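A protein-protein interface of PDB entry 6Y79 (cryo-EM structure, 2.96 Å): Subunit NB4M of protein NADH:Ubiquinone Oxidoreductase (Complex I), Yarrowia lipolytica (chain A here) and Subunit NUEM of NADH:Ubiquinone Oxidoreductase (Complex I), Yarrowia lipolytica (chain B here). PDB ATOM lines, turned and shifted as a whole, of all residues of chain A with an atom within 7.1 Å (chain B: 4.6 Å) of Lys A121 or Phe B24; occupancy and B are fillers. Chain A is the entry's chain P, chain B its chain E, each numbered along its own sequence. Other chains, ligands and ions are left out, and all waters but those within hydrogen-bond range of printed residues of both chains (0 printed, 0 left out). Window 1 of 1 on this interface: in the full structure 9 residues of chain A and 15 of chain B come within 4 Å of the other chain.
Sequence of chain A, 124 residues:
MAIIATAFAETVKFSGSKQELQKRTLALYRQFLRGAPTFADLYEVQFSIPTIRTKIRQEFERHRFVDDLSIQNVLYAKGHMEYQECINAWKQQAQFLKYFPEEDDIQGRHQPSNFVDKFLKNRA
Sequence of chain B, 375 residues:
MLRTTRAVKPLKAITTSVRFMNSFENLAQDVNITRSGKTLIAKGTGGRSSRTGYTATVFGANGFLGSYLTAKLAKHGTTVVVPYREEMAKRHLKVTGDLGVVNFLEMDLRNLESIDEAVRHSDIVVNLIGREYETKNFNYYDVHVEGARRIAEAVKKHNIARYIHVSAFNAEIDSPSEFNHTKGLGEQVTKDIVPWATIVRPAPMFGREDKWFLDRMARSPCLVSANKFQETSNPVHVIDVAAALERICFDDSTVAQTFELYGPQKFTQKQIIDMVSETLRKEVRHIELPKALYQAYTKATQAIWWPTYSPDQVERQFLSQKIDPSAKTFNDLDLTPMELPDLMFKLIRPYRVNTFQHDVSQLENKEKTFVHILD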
ATOM      1  N   GLN A 107     -25.813  10.132   1.926  1.00  0.00           N
ATOM      2  CA  GLN A 107     -26.639   9.324   1.036  1.00  0.00           C
ATOM      3  C   GLN A 107     -26.213   7.861   1.026  1.00  0.00           C
ATOM      4  O   GLN A 107     -26.993   7.006   0.592  1.00  0.00           O
ATOM      5  CB  GLN A 107     -26.632   9.919  -0.372  1.00  0.00           C
ATOM      6  CG  GLN A 107     -27.244  11.327  -0.443  1.00  0.00           C
ATOM      7  CD  GLN A 107     -27.906  11.634  -1.783  1.00  0.00           C
ATOM      8  OE1 GLN A 107     -27.401  11.258  -2.840  1.00  0.00           O
ATOM      9  NE2 GLN A 107     -29.041  12.329  -1.738  1.00  0.00           N
ATOM     10  N   ARG A 109     -22.790   4.684   1.506  1.00  0.00           N
ATOM     11  CA  ARG A 109     -21.410   4.314   1.235  1.00  0.00           C
ATOM     12  C   ARG A 109     -21.037   4.564  -0.206  1.00  0.00           C
ATOM     13  O   ARG A 109     -21.819   5.087  -1.005  1.00  0.00           O
ATOM     14  CB  ARG A 109     -21.159   2.836   1.449  1.00  0.00           C
ATOM     15  CG  ARG A 109     -21.278   2.319   2.830  1.00  0.00           C
ATOM     16  CD  ARG A 109     -21.154   0.795   2.735  1.00  0.00           C
ATOM     17  NE  ARG A 109     -19.821   0.298   2.613  1.00  0.00           N
ATOM     18  CZ  ARG A 109     -19.014   0.049   3.634  1.00  0.00           C
ATOM     19  NH1 ARG A 109     -17.790  -0.459   3.459  1.00  0.00           N
ATOM     20  NH2 ARG A 109     -19.437   0.326   4.840  1.00  0.00           N
ATOM     21  N   HIS A 110     -19.816   4.118  -0.516  1.00  0.00           N
ATOM     22  CA  HIS A 110     -19.375   3.766  -1.863  1.00  0.00           C
ATOM     23  C   HIS A 110     -19.495   4.951  -2.818  1.00  0.00           C
ATOM     24  O   HIS A 110     -20.156   4.883  -3.854  1.00  0.00           O
ATOM     25  CB  HIS A 110     -20.140   2.547  -2.385  1.00  0.00           C
ATOM     26  CG  HIS A 110     -19.838   1.273  -1.653  1.00  0.00           C
ATOM     27  ND1 HIS A 110     -18.580   0.711  -1.622  1.00  0.00           N
ATOM     28  CD2 HIS A 110     -20.641   0.430  -0.962  1.00  0.00           C
ATOM     29  CE1 HIS A 110     -18.616  -0.408  -0.920  1.00  0.00           C
ATOM     30  NE2 HIS A 110     -19.855  -0.603  -0.510  1.00  0.00           N
ATOM     31  N   GLN A 111     -18.901   6.062  -2.422  1.00  0.00           N
ATOM     32  CA  GLN A 111     -18.875   7.234  -3.273  1.00  0.00           C
ATOM     33  C   GLN A 111     -17.821   7.026  -4.347  1.00  0.00           C
ATOM     34  O   GLN A 111     -16.639   6.869  -4.016  1.00  0.00           O
ATOM     35  CB  GLN A 111     -18.572   8.482  -2.454  1.00  0.00           C
ATOM     36  CG  GLN A 111     -19.609   8.790  -1.386  1.00  0.00           C
ATOM     37  CD  GLN A 111     -20.911   9.307  -1.967  1.00  0.00           C
ATOM     38  OE1 GLN A 111     -20.931   9.903  -3.045  1.00  0.00           O
ATOM     39  NE2 GLN A 111     -22.006   9.085  -1.252  1.00  0.00           N
ATOM     40  N   PRO A 112     -18.189   7.001  -5.629  1.00  0.00           N
ATOM     41  CA  PRO A 112     -17.198   6.734  -6.680  1.00  0.00           C
ATOM     42  C   PRO A 112     -16.315   7.952  -6.925  1.00  0.00           C
ATOM     43  O   PRO A 112     -16.799   9.034  -7.260  1.00  0.00           O
ATOM     44  CB  PRO A 112     -18.060   6.398  -7.903  1.00  0.00           C
ATOM     45  CG  PRO A 112     -19.377   7.030  -7.642  1.00  0.00           C
ATOM     46  CD  PRO A 112     -19.556   7.142  -6.160  1.00  0.00           C
ATOM     47  N   VAL A 116     -12.117   3.337 -11.394  1.00  0.00           N
ATOM     48  CA  VAL A 116     -12.518   1.937 -11.278  1.00  0.00           C
ATOM     49  C   VAL A 116     -13.808   1.811 -10.473  1.00  0.00           C
ATOM     50  O   VAL A 116     -14.707   1.040 -10.829  1.00  0.00           O
ATOM     51  CB  VAL A 116     -11.369   1.103 -10.687  1.00  0.00           C
ATOM     52  CG1 VAL A 116     -11.828  -0.291 -10.314  1.00  0.00           C
ATOM     53  CG2 VAL A 116     -10.257   1.005 -11.700  1.00  0.00           C
ATOM     54  N   ASP A 117     -13.946   2.582  -9.394  1.00  0.00           N
ATOM     55  CA  ASP A 117     -15.205   2.516  -8.663  1.00  0.00           C
ATOM     56  C   ASP A 117     -16.305   3.324  -9.334  1.00  0.00           C
ATOM     57  O   ASP A 117     -17.477   3.159  -8.981  1.00  0.00           O
ATOM     58  CB  ASP A 117     -15.004   2.946  -7.214  1.00  0.00           C
ATOM     59  CG  ASP A 117     -14.264   1.898  -6.403  1.00  0.00           C
ATOM     60  OD1 ASP A 117     -14.324   0.712  -6.784  1.00  0.00           O
ATOM     61  OD2 ASP A 117     -13.647   2.249  -5.377  1.00  0.00           O
ATOM     62  N   LYS A 118     -15.957   4.188 -10.289  1.00  0.00           N
ATOM     63  CA  LYS A 118     -16.950   4.650 -11.251  1.00  0.00           C
ATOM     64  C   LYS A 118     -17.268   3.561 -12.262  1.00  0.00           C
ATOM     65  O   LYS A 118     -18.385   3.502 -12.781  1.00  0.00           O
ATOM     66  CB  LYS A 118     -16.455   5.899 -11.979  1.00  0.00           C
ATOM     67  CG  LYS A 118     -16.614   7.191 -11.211  1.00  0.00           C
ATOM     68  CD  LYS A 118     -16.396   8.399 -12.111  1.00  0.00           C
ATOM     69  CE  LYS A 118     -14.996   8.395 -12.710  1.00  0.00           C
ATOM     70  NZ  LYS A 118     -14.646   9.681 -13.371  1.00  0.00           N
ATOM     71  N   PHE A 119     -16.301   2.690 -12.540  1.00  0.00           N
ATOM     72  CA  PHE A 119     -16.441   1.661 -13.560  1.00  0.00           C
ATOM     73  C   PHE A 119     -17.197   0.454 -13.037  1.00  0.00           C
ATOM     74  O   PHE A 119     -17.916  -0.203 -13.796  1.00  0.00           O
ATOM     75  CB  PHE A 119     -15.060   1.236 -14.057  1.00  0.00           C
ATOM     76  CG  PHE A 119     -15.090   0.147 -15.082  1.00  0.00           C
ATOM     77  CD1 PHE A 119     -15.407   0.436 -16.393  1.00  0.00           C
ATOM     78  CD2 PHE A 119     -14.794  -1.165 -14.740  1.00  0.00           C
ATOM     79  CE1 PHE A 119     -15.434  -0.558 -17.343  1.00  0.00           C
ATOM     80  CE2 PHE A 119     -14.825  -2.162 -15.685  1.00  0.00           C
ATOM     81  CZ  PHE A 119     -15.142  -1.858 -16.987  1.00  0.00           C
ATOM     82  N   LEU A 120     -17.031   0.136 -11.752  1.00  0.00           N
ATOM     83  CA  LEU A 120     -17.661  -1.048 -11.185  1.00  0.00           C
ATOM     84  C   LEU A 120     -19.174  -0.934 -11.138  1.00  0.00           C
ATOM     85  O   LEU A 120     -19.861  -1.957 -11.149  1.00  0.00           O
ATOM     86  CB  LEU A 120     -17.127  -1.310  -9.782  1.00  0.00           C
ATOM     87  CG  LEU A 120     -15.704  -1.840  -9.636  1.00  0.00           C
ATOM     88  CD1 LEU A 120     -15.439  -2.111  -8.184  1.00  0.00           C
ATOM     89  CD2 LEU A 120     -15.499  -3.078 -10.449  1.00  0.00           C
ATOM     90  N   LYS A 121     -19.702   0.285 -11.105  1.00  0.00           N
ATOM     91  CA  LYS A 121     -21.136   0.517 -11.150  1.00  0.00           C
ATOM     92  C   LYS A 121     -21.570   1.234 -12.421  1.00  0.00           C
ATOM     93  O   LYS A 121     -22.686   1.753 -12.451  1.00  0.00           O
ATOM     94  CB  LYS A 121     -21.565   1.323  -9.925  1.00  0.00           C
ATOM     95  CG  LYS A 121     -20.855   2.644  -9.808  1.00  0.00           C
ATOM     96  CD  LYS A 121     -21.370   3.445  -8.635  1.00  0.00           C
ATOM     97  CE  LYS A 121     -20.884   2.878  -7.322  1.00  0.00           C
ATOM     98  NZ  LYS A 121     -21.230   3.783  -6.197  1.00  0.00           N
ATOM     99  N   ASN A 122     -20.688   1.296 -13.435  1.00  0.00           N
ATOM    100  CA  ASN A 122     -20.695   2.072 -14.688  1.00  0.00           C
ATOM    101  C   ASN A 122     -21.405   3.414 -14.555  1.00  0.00           C
ATOM    102  O   ASN A 122     -22.296   3.744 -15.342  1.00  0.00           O
ATOM    103  CB  ASN A 122     -21.169   1.252 -15.921  1.00  0.00           C
ATOM    104  CG  ASN A 122     -22.611   0.749 -15.873  1.00  0.00           C
ATOM    105  OD1 ASN A 122     -23.397   1.084 -15.012  1.00  0.00           O
ATOM    106  ND2 ASN A 122     -22.956  -0.062 -16.862  1.00  0.00           N
ATOM    107  N   ARG A 123     -20.997   4.174 -13.536  1.00  0.00           N
ATOM    108  CA  ARG A 123     -21.401   5.519 -13.125  1.00  0.00           C
ATOM    109  C   ARG A 123     -22.803   5.548 -12.524  1.00  0.00           C
ATOM    110  O   ARG A 123     -23.251   6.638 -12.135  1.00  0.00           O
ATOM    111  CB  ARG A 123     -21.316   6.561 -14.253  1.00  0.00           C
ATOM    112  CG  ARG A 123     -19.922   7.070 -14.524  1.00  0.00           C
ATOM    113  CD  ARG A 123     -19.154   6.134 -15.428  1.00  0.00           C
ATOM    114  NE  ARG A 123     -17.852   6.682 -15.773  1.00  0.00           N
ATOM    115  CZ  ARG A 123     -16.821   5.950 -16.173  1.00  0.00           C
ATOM    116  NH1 ARG A 123     -16.936   4.635 -16.268  1.00  0.00           N
ATOM    117  NH2 ARG A 123     -15.670   6.537 -16.465  1.00  0.00           N
ATOM    118  N   ALA A 124     -23.482   4.399 -12.422  1.00  0.00           N
ATOM    119  CA  ALA A 124     -24.811   4.172 -11.825  1.00  0.00           C
ATOM    120  C   ALA A 124     -25.847   5.244 -12.112  1.00  0.00           C
ATOM    121  O   ALA A 124     -25.930   5.739 -13.230  1.00  0.00           O
ATOM    122  CB  ALA A 124     -24.679   3.973 -10.318  1.00  0.00           C
ATOM    123  N   SER B  23     -27.614   7.719  -7.959  1.00  0.00           N
ATOM    124  CA  SER B  23     -26.559   6.716  -7.976  1.00  0.00           C
ATOM    125  C   SER B  23     -26.810   5.697  -6.876  1.00  0.00           C
ATOM    126  O   SER B  23     -27.322   6.027  -5.805  1.00  0.00           O
ATOM    127  CB  SER B  23     -25.171   7.353  -7.799  1.00  0.00           C
ATOM    128  OG  SER B  23     -24.141   6.445  -8.107  1.00  0.00           O
ATOM    129  N   PHE B  24     -26.422   4.453  -7.146  1.00  0.00           N
ATOM    130  CA  PHE B  24     -26.482   3.384  -6.159  1.00  0.00           C
ATOM    131  C   PHE B  24     -25.407   3.573  -5.100  1.00  0.00           C
ATOM    132  O   PHE B  24     -24.262   3.165  -5.314  1.00  0.00           O
ATOM    133  CB  PHE B  24     -26.268   2.024  -6.820  1.00  0.00           C
ATOM    134  CG  PHE B  24     -27.357   1.612  -7.752  1.00  0.00           C
ATOM    135  CD1 PHE B  24     -28.682   1.838  -7.445  1.00  0.00           C
ATOM    136  CD2 PHE B  24     -27.047   0.983  -8.941  1.00  0.00           C
ATOM    137  CE1 PHE B  24     -29.677   1.444  -8.313  1.00  0.00           C
ATOM    138  CE2 PHE B  24     -28.034   0.591  -9.810  1.00  0.00           C
ATOM    139  CZ  PHE B  24     -29.348   0.819  -9.494  1.00  0.00           C
ATOM    140  N   GLU B  25     -25.739   4.177  -3.958  1.00  0.00           N
ATOM    141  CA  GLU B  25     -24.712   4.326  -2.932  1.00  0.00           C
ATOM    142  C   GLU B  25     -24.596   3.086  -2.053  1.00  0.00           C
ATOM    143  O   GLU B  25     -23.520   2.817  -1.513  1.00  0.00           O
ATOM    144  CB  GLU B  25     -24.963   5.572  -2.083  1.00  0.00           C
ATOM    145  CG  GLU B  25     -25.197   6.823  -2.902  1.00  0.00           C
ATOM    146  CD  GLU B  25     -26.637   7.267  -2.825  1.00  0.00           C
ATOM    147  OE1 GLU B  25     -27.445   6.470  -2.323  1.00  0.00           O
ATOM    148  OE2 GLU B  25     -26.958   8.372  -3.296  1.00  0.00           O
ATOM    149  N   ASN B  26     -25.672   2.306  -1.905  1.00  0.00           N
ATOM    150  CA  ASN B  26     -25.595   1.122  -1.053  1.00  0.00           C
ATOM    151  C   ASN B  26     -24.752   0.020  -1.682  1.00  0.00           C
ATOM    152  O   ASN B  26     -24.216  -0.836  -0.971  1.00  0.00           O
ATOM    153  CB  ASN B  26     -26.998   0.594  -0.723  1.00  0.00           C
ATOM    154  CG  ASN B  26     -27.849   0.302  -1.961  1.00  0.00           C
ATOM    155  OD1 ASN B  26     -27.391   0.380  -3.100  1.00  0.00           O
ATOM    156  ND2 ASN B  26     -29.108  -0.044  -1.727  1.00  0.00           N
ATOM    157  N   LEU B  27     -24.628   0.033  -3.001  1.00  0.00           N
ATOM    158  CA  LEU B  27     -23.913  -0.998  -3.731  1.00  0.00           C
ATOM    159  C   LEU B  27     -22.451  -0.625  -3.909  1.00  0.00           C
ATOM    160  O   LEU B  27     -22.116   0.537  -4.151  1.00  0.00           O
ATOM    161  CB  LEU B  27     -24.549  -1.209  -5.101  1.00  0.00           C
ATOM    162  CG  LEU B  27     -25.902  -1.900  -5.169  1.00  0.00           C
ATOM    163  CD1 LEU B  27     -26.300  -2.056  -6.617  1.00  0.00           C
ATOM    164  CD2 LEU B  27     -25.832  -3.243  -4.485  1.00  0.00           C
ATOM    165  N   ALA B  28     -21.581  -1.625  -3.791  1.00  0.00           N
ATOM    166  CA  ALA B  28     -20.191  -1.427  -4.168  1.00  0.00           C
ATOM    167  C   ALA B  28     -20.043  -1.326  -5.675  1.00  0.00           C
ATOM    168  O   ALA B  28     -19.143  -0.636  -6.167  1.00  0.00           O
ATOM    169  CB  ALA B  28     -19.332  -2.572  -3.638  1.00  0.00           C
ATOM    170  N   GLN B  29     -20.901  -2.021  -6.423  1.00  0.00           N
ATOM    171  CA  GLN B  29     -20.746  -2.196  -7.863  1.00  0.00           C
ATOM    172  C   GLN B  29     -22.115  -2.225  -8.522  1.00  0.00           C
ATOM    173  O   GLN B  29     -23.117  -1.782  -7.959  1.00  0.00           O
ATOM    174  CB  GLN B  29     -20.050  -3.506  -8.226  1.00  0.00           C
ATOM    175  CG  GLN B  29     -18.767  -3.817  -7.565  1.00  0.00           C
ATOM    176  CD  GLN B  29     -18.357  -5.186  -7.925  1.00  0.00           C
ATOM    177  OE1 GLN B  29     -18.984  -5.807  -8.777  1.00  0.00           O
ATOM    178  NE2 GLN B  29     -17.320  -5.689  -7.281  1.00  0.00           N
ATOM    179  N   ASP B  30     -22.138  -2.741  -9.750  1.00  0.00           N
ATOM    180  CA  ASP B  30     -23.363  -3.112 -10.445  1.00  0.00           C
ATOM    181  C   ASP B  30     -23.659  -4.604 -10.275  1.00  0.00           C
ATOM    182  O   ASP B  30     -24.651  -4.976  -9.642  1.00  0.00           O
ATOM    183  CB  ASP B  30     -23.217  -2.733 -11.927  1.00  0.00           C
ATOM    184  CG  ASP B  30     -24.500  -2.904 -12.738  1.00  0.00           C
ATOM    185  OD1 ASP B  30     -25.521  -3.410 -12.227  1.00  0.00           O
ATOM    186  OD2 ASP B  30     -24.497  -2.492 -13.914  1.00  0.00           O
ATOM    187  N   ALA B  42     -27.819  -5.039 -11.407  1.00  0.00           N
ATOM    188  CA  ALA B  42     -28.634  -3.878 -11.089  1.00  0.00           C
ATOM    189  C   ALA B  42     -28.879  -3.058 -12.347  1.00  0.00           C
ATOM    190  O   ALA B  42     -28.058  -3.026 -13.263  1.00  0.00           O
ATOM    191  CB  ALA B  42     -27.969  -3.028 -10.010  1.00  0.00           C
ATOM    192  N   LYS B  43     -30.033  -2.422 -12.412  1.00  0.00           N
ATOM    193  CA  LYS B  43     -30.470  -1.798 -13.647  1.00  0.00           C
ATOM    194  C   LYS B  43     -30.620  -0.299 -13.467  1.00  0.00           C
ATOM    195  O   LYS B  43     -31.117   0.170 -12.449  1.00  0.00           O
ATOM    196  CB  LYS B  43     -31.789  -2.400 -14.110  1.00  0.00           C
ATOM    197  CG  LYS B  43     -31.665  -3.840 -14.533  1.00  0.00           C
ATOM    198  CD  LYS B  43     -32.940  -4.308 -15.178  1.00  0.00           C
ATOM    199  CE  LYS B  43     -34.075  -4.286 -14.182  1.00  0.00           C
ATOM    200  NZ  LYS B  43     -35.315  -4.842 -14.769  1.00  0.00           N
ATOM    201  N   GLY B  44     -30.164   0.440 -14.454  1.00  0.00           N
ATOM    202  CA  GLY B  44     -30.384   1.860 -14.469  1.00  0.00           C
ATOM    203  C   GLY B  44     -29.496   2.655 -13.536  1.00  0.00           C
ATOM    204  O   GLY B  44     -28.494   2.186 -13.006  1.00  0.00           O
ATOM    205  N   THR B  45     -29.899   3.906 -13.352  1.00  0.00           N
ATOM    206  CA  THR B  45     -29.259   4.790 -12.392  1.00  0.00           C
ATOM    207  C   THR B  45     -29.823   4.484 -11.011  1.00  0.00           C
ATOM    208  O   THR B  45     -30.589   3.539 -10.828  1.00  0.00           O
ATOM    209  CB  THR B  45     -29.450   6.249 -12.797  1.00  0.00           C
ATOM    210  OG1 THR B  45     -30.835   6.597 -12.713  1.00  0.00           O
ATOM    211  CG2 THR B  45     -28.991   6.460 -14.219  1.00  0.00           C
ATOM    212  N   GLY B  46     -29.463   5.259 -10.016  1.00  0.00           N
ATOM    213  CA  GLY B  46     -30.068   5.060  -8.720  1.00  0.00           C
ATOM    214  C   GLY B  46     -31.473   5.613  -8.678  1.00  0.00           C
ATOM    215  O   GLY B  46     -31.966   6.228  -9.620  1.00  0.00           O
ATOM    216  N   SER B  50     -35.664   2.508 -10.510  1.00  0.00           N
ATOM    217  CA  SER B  50     -34.748   1.440 -10.876  1.00  0.00           C
ATOM    218  C   SER B  50     -34.661   0.394  -9.777  1.00  0.00           C
ATOM    219  O   SER B  50     -35.193   0.557  -8.682  1.00  0.00           O
ATOM    220  CB  SER B  50     -33.367   1.992 -11.164  1.00  0.00           C
ATOM    221  OG  SER B  50     -32.775   2.520 -10.000  1.00  0.00           O
ATOM    222  N   ARG B  51     -33.964  -0.696 -10.090  1.00  0.00           N
ATOM    223  CA  ARG B  51     -33.953  -1.891  -9.261  1.00  0.00           C
ATOM    224  C   ARG B  51     -32.528  -2.368  -9.047  1.00  0.00           C
ATOM    225  O   ARG B  51     -31.740  -2.429  -9.991  1.00  0.00           O
ATOM    226  CB  ARG B  51     -34.759  -3.021  -9.901  1.00  0.00           C
ATOM    227  CG  ARG B  51     -36.179  -2.667 -10.238  1.00  0.00           C
ATOM    228  CD  ARG B  51     -36.950  -2.349  -8.999  1.00  0.00           C
ATOM    229  NE  ARG B  51     -38.377  -2.271  -9.297  1.00  0.00           N
ATOM    230  CZ  ARG B  51     -39.050  -1.145  -9.483  1.00  0.00           C
ATOM    231  NH1 ARG B  51     -40.335  -1.196  -9.757  1.00  0.00           N
ATOM    232  NH2 ARG B  51     -38.443   0.026  -9.367  1.00  0.00           N
ATOM    233  N   THR B  52     -32.206  -2.723  -7.804  1.00  0.00           N
ATOM    234  CA  THR B  52     -30.891  -3.276  -7.500  1.00  0.00           C
ATOM    235  C   THR B  52     -30.815  -4.770  -7.777  1.00  0.00           C
ATOM    236  O   THR B  52     -29.795  -5.254  -8.273  1.00  0.00           O
ATOM    237  CB  THR B  52     -30.521  -3.002  -6.041  1.00  0.00           C
ATOM    238  OG1 THR B  52     -31.352  -3.783  -5.178  1.00  0.00           O
ATOM    239  CG2 THR B  52     -30.717  -1.545  -5.716  1.00  0.00           C
ATOM    240  N   HIS B  76     -33.753   2.424  -3.172  1.00  0.00           N
ATOM    241  CA  HIS B  76     -32.972   2.147  -4.365  1.00  0.00           C
ATOM    242  C   HIS B  76     -33.566   1.068  -5.240  1.00  0.00           C
ATOM    243  O   HIS B  76     -33.021   0.795  -6.310  1.00  0.00           O
ATOM    244  CB  HIS B  76     -31.553   1.763  -3.974  1.00  0.00           C
ATOM    245  CG  HIS B  76     -30.800   2.898  -3.386  1.00  0.00           C
ATOM    246  ND1 HIS B  76     -30.448   3.999  -4.130  1.00  0.00           N
ATOM    247  CD2 HIS B  76     -30.376   3.138  -2.125  1.00  0.00           C
ATOM    248  CE1 HIS B  76     -29.823   4.865  -3.357  1.00  0.00           C
ATOM    249  NE2 HIS B  76     -29.762   4.365  -2.137  1.00  0.00           N
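The backbone carbonyl oxygen of Glu B25 sits close to the backbone carbonyl oxygen of Arg A109 (2.9 Å).
The backbone carbonyl oxygen of Phe B24 sits at hydrogen-bond distance from the side-chain amino group of Lys A121, at 3.2 Å.
O of Leu A120 lies within hydrogen-bond range of N of Asp B30, at 2.8 Å.
The side-chain carboxylate (OE2) of Glu B25 lies close to the side-chain amide oxygen (OE1) of Gln A107 (3.0 Å).
O of Thr B45 lies within hydrogen-bond range of OG of Ser B50 (2.6 Å).
The backbone carbonyl oxygen of His A110 is in hydrogen-bond range of the side-chain amino group of Lys A121 (2.8 Å).
The side-chain carboxylate (OD1) of Asp B30 lies within hydrogen-bond range of the backbone NH (N) of Ala B42 (2.9 Å).
The guanidinium group (NE) of Arg A109 lies within hydrogen-bond range of a ring nitrogen (NE2) of His A110.
OE1 of Glu B25 sits close to NE2 of His B76 (3.1 Å).
Among the printed residues, pairs that only touch across the chains: Ala A124 with Thr B45 (3.3 Å), Leu A120 with Gln B29 (3.3 Å), His A110 with Leu B27 (3.3 Å), Ala A124 with Ser B23 (3.4 Å), His A110 with Glu B25 (3.5 Å), His A110 with Ala B28 (3.5 Å), Ala A124 with Phe B24 (3.7 Å), Lys A121 with Asp B30 (3.7 Å), His A110 with Asn B26 (3.8 Å), Lys A121 with Gln B29 (3.9 Å), Asn A122 with Asp B30 (3.9 Å) and Lys A121 with Leu B27 (3.9 Å).
Phe B24 touches two residues of chain A.
Of the printed residues of chain A, Asp B30 touches Leu A120 (2.8 Å), Lys A121 (3.7 Å) and Asn A122 (3.9 Å).
Of the printed residues of chain B, Arg A109 touches Glu B25.
Printed residues of chain A within 4 Å of Ser B23: Ala A124 (3.4 Å).
Printed residues of chain A within 4 Å of Leu B27: His A110 and Lys A121.
The nearest printed residue of chain B that does not touch Lys A121 is Ala B28 (4.1 Å).
The nearest printed residue of chain A that does not touch Glu B25 is Gln A111 (4.2 Å).
Printed residues of chain A that touch a printed residue of chain B: Gln A107, Arg A109, His A110, Leu A120, Lys A121, Asn A122 and Ala A124.
Printed residues of chain B that touch a printed residue of chain A: Ser B23, Phe B24, Glu B25, Asn B26, Leu B27, Ala B28, Gln B29, Asp B30 and Thr B45.
Hydrophobic or aromatic side chains of chain B that line the printed part of chain A: Ala B28.
Among the printed residues, 16 pairs touch across the chains.
Among the printed residues, no Asp or Glu carboxylate lies within 4 Å of a Lys or Arg side-chain nitrogen of the other chain.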
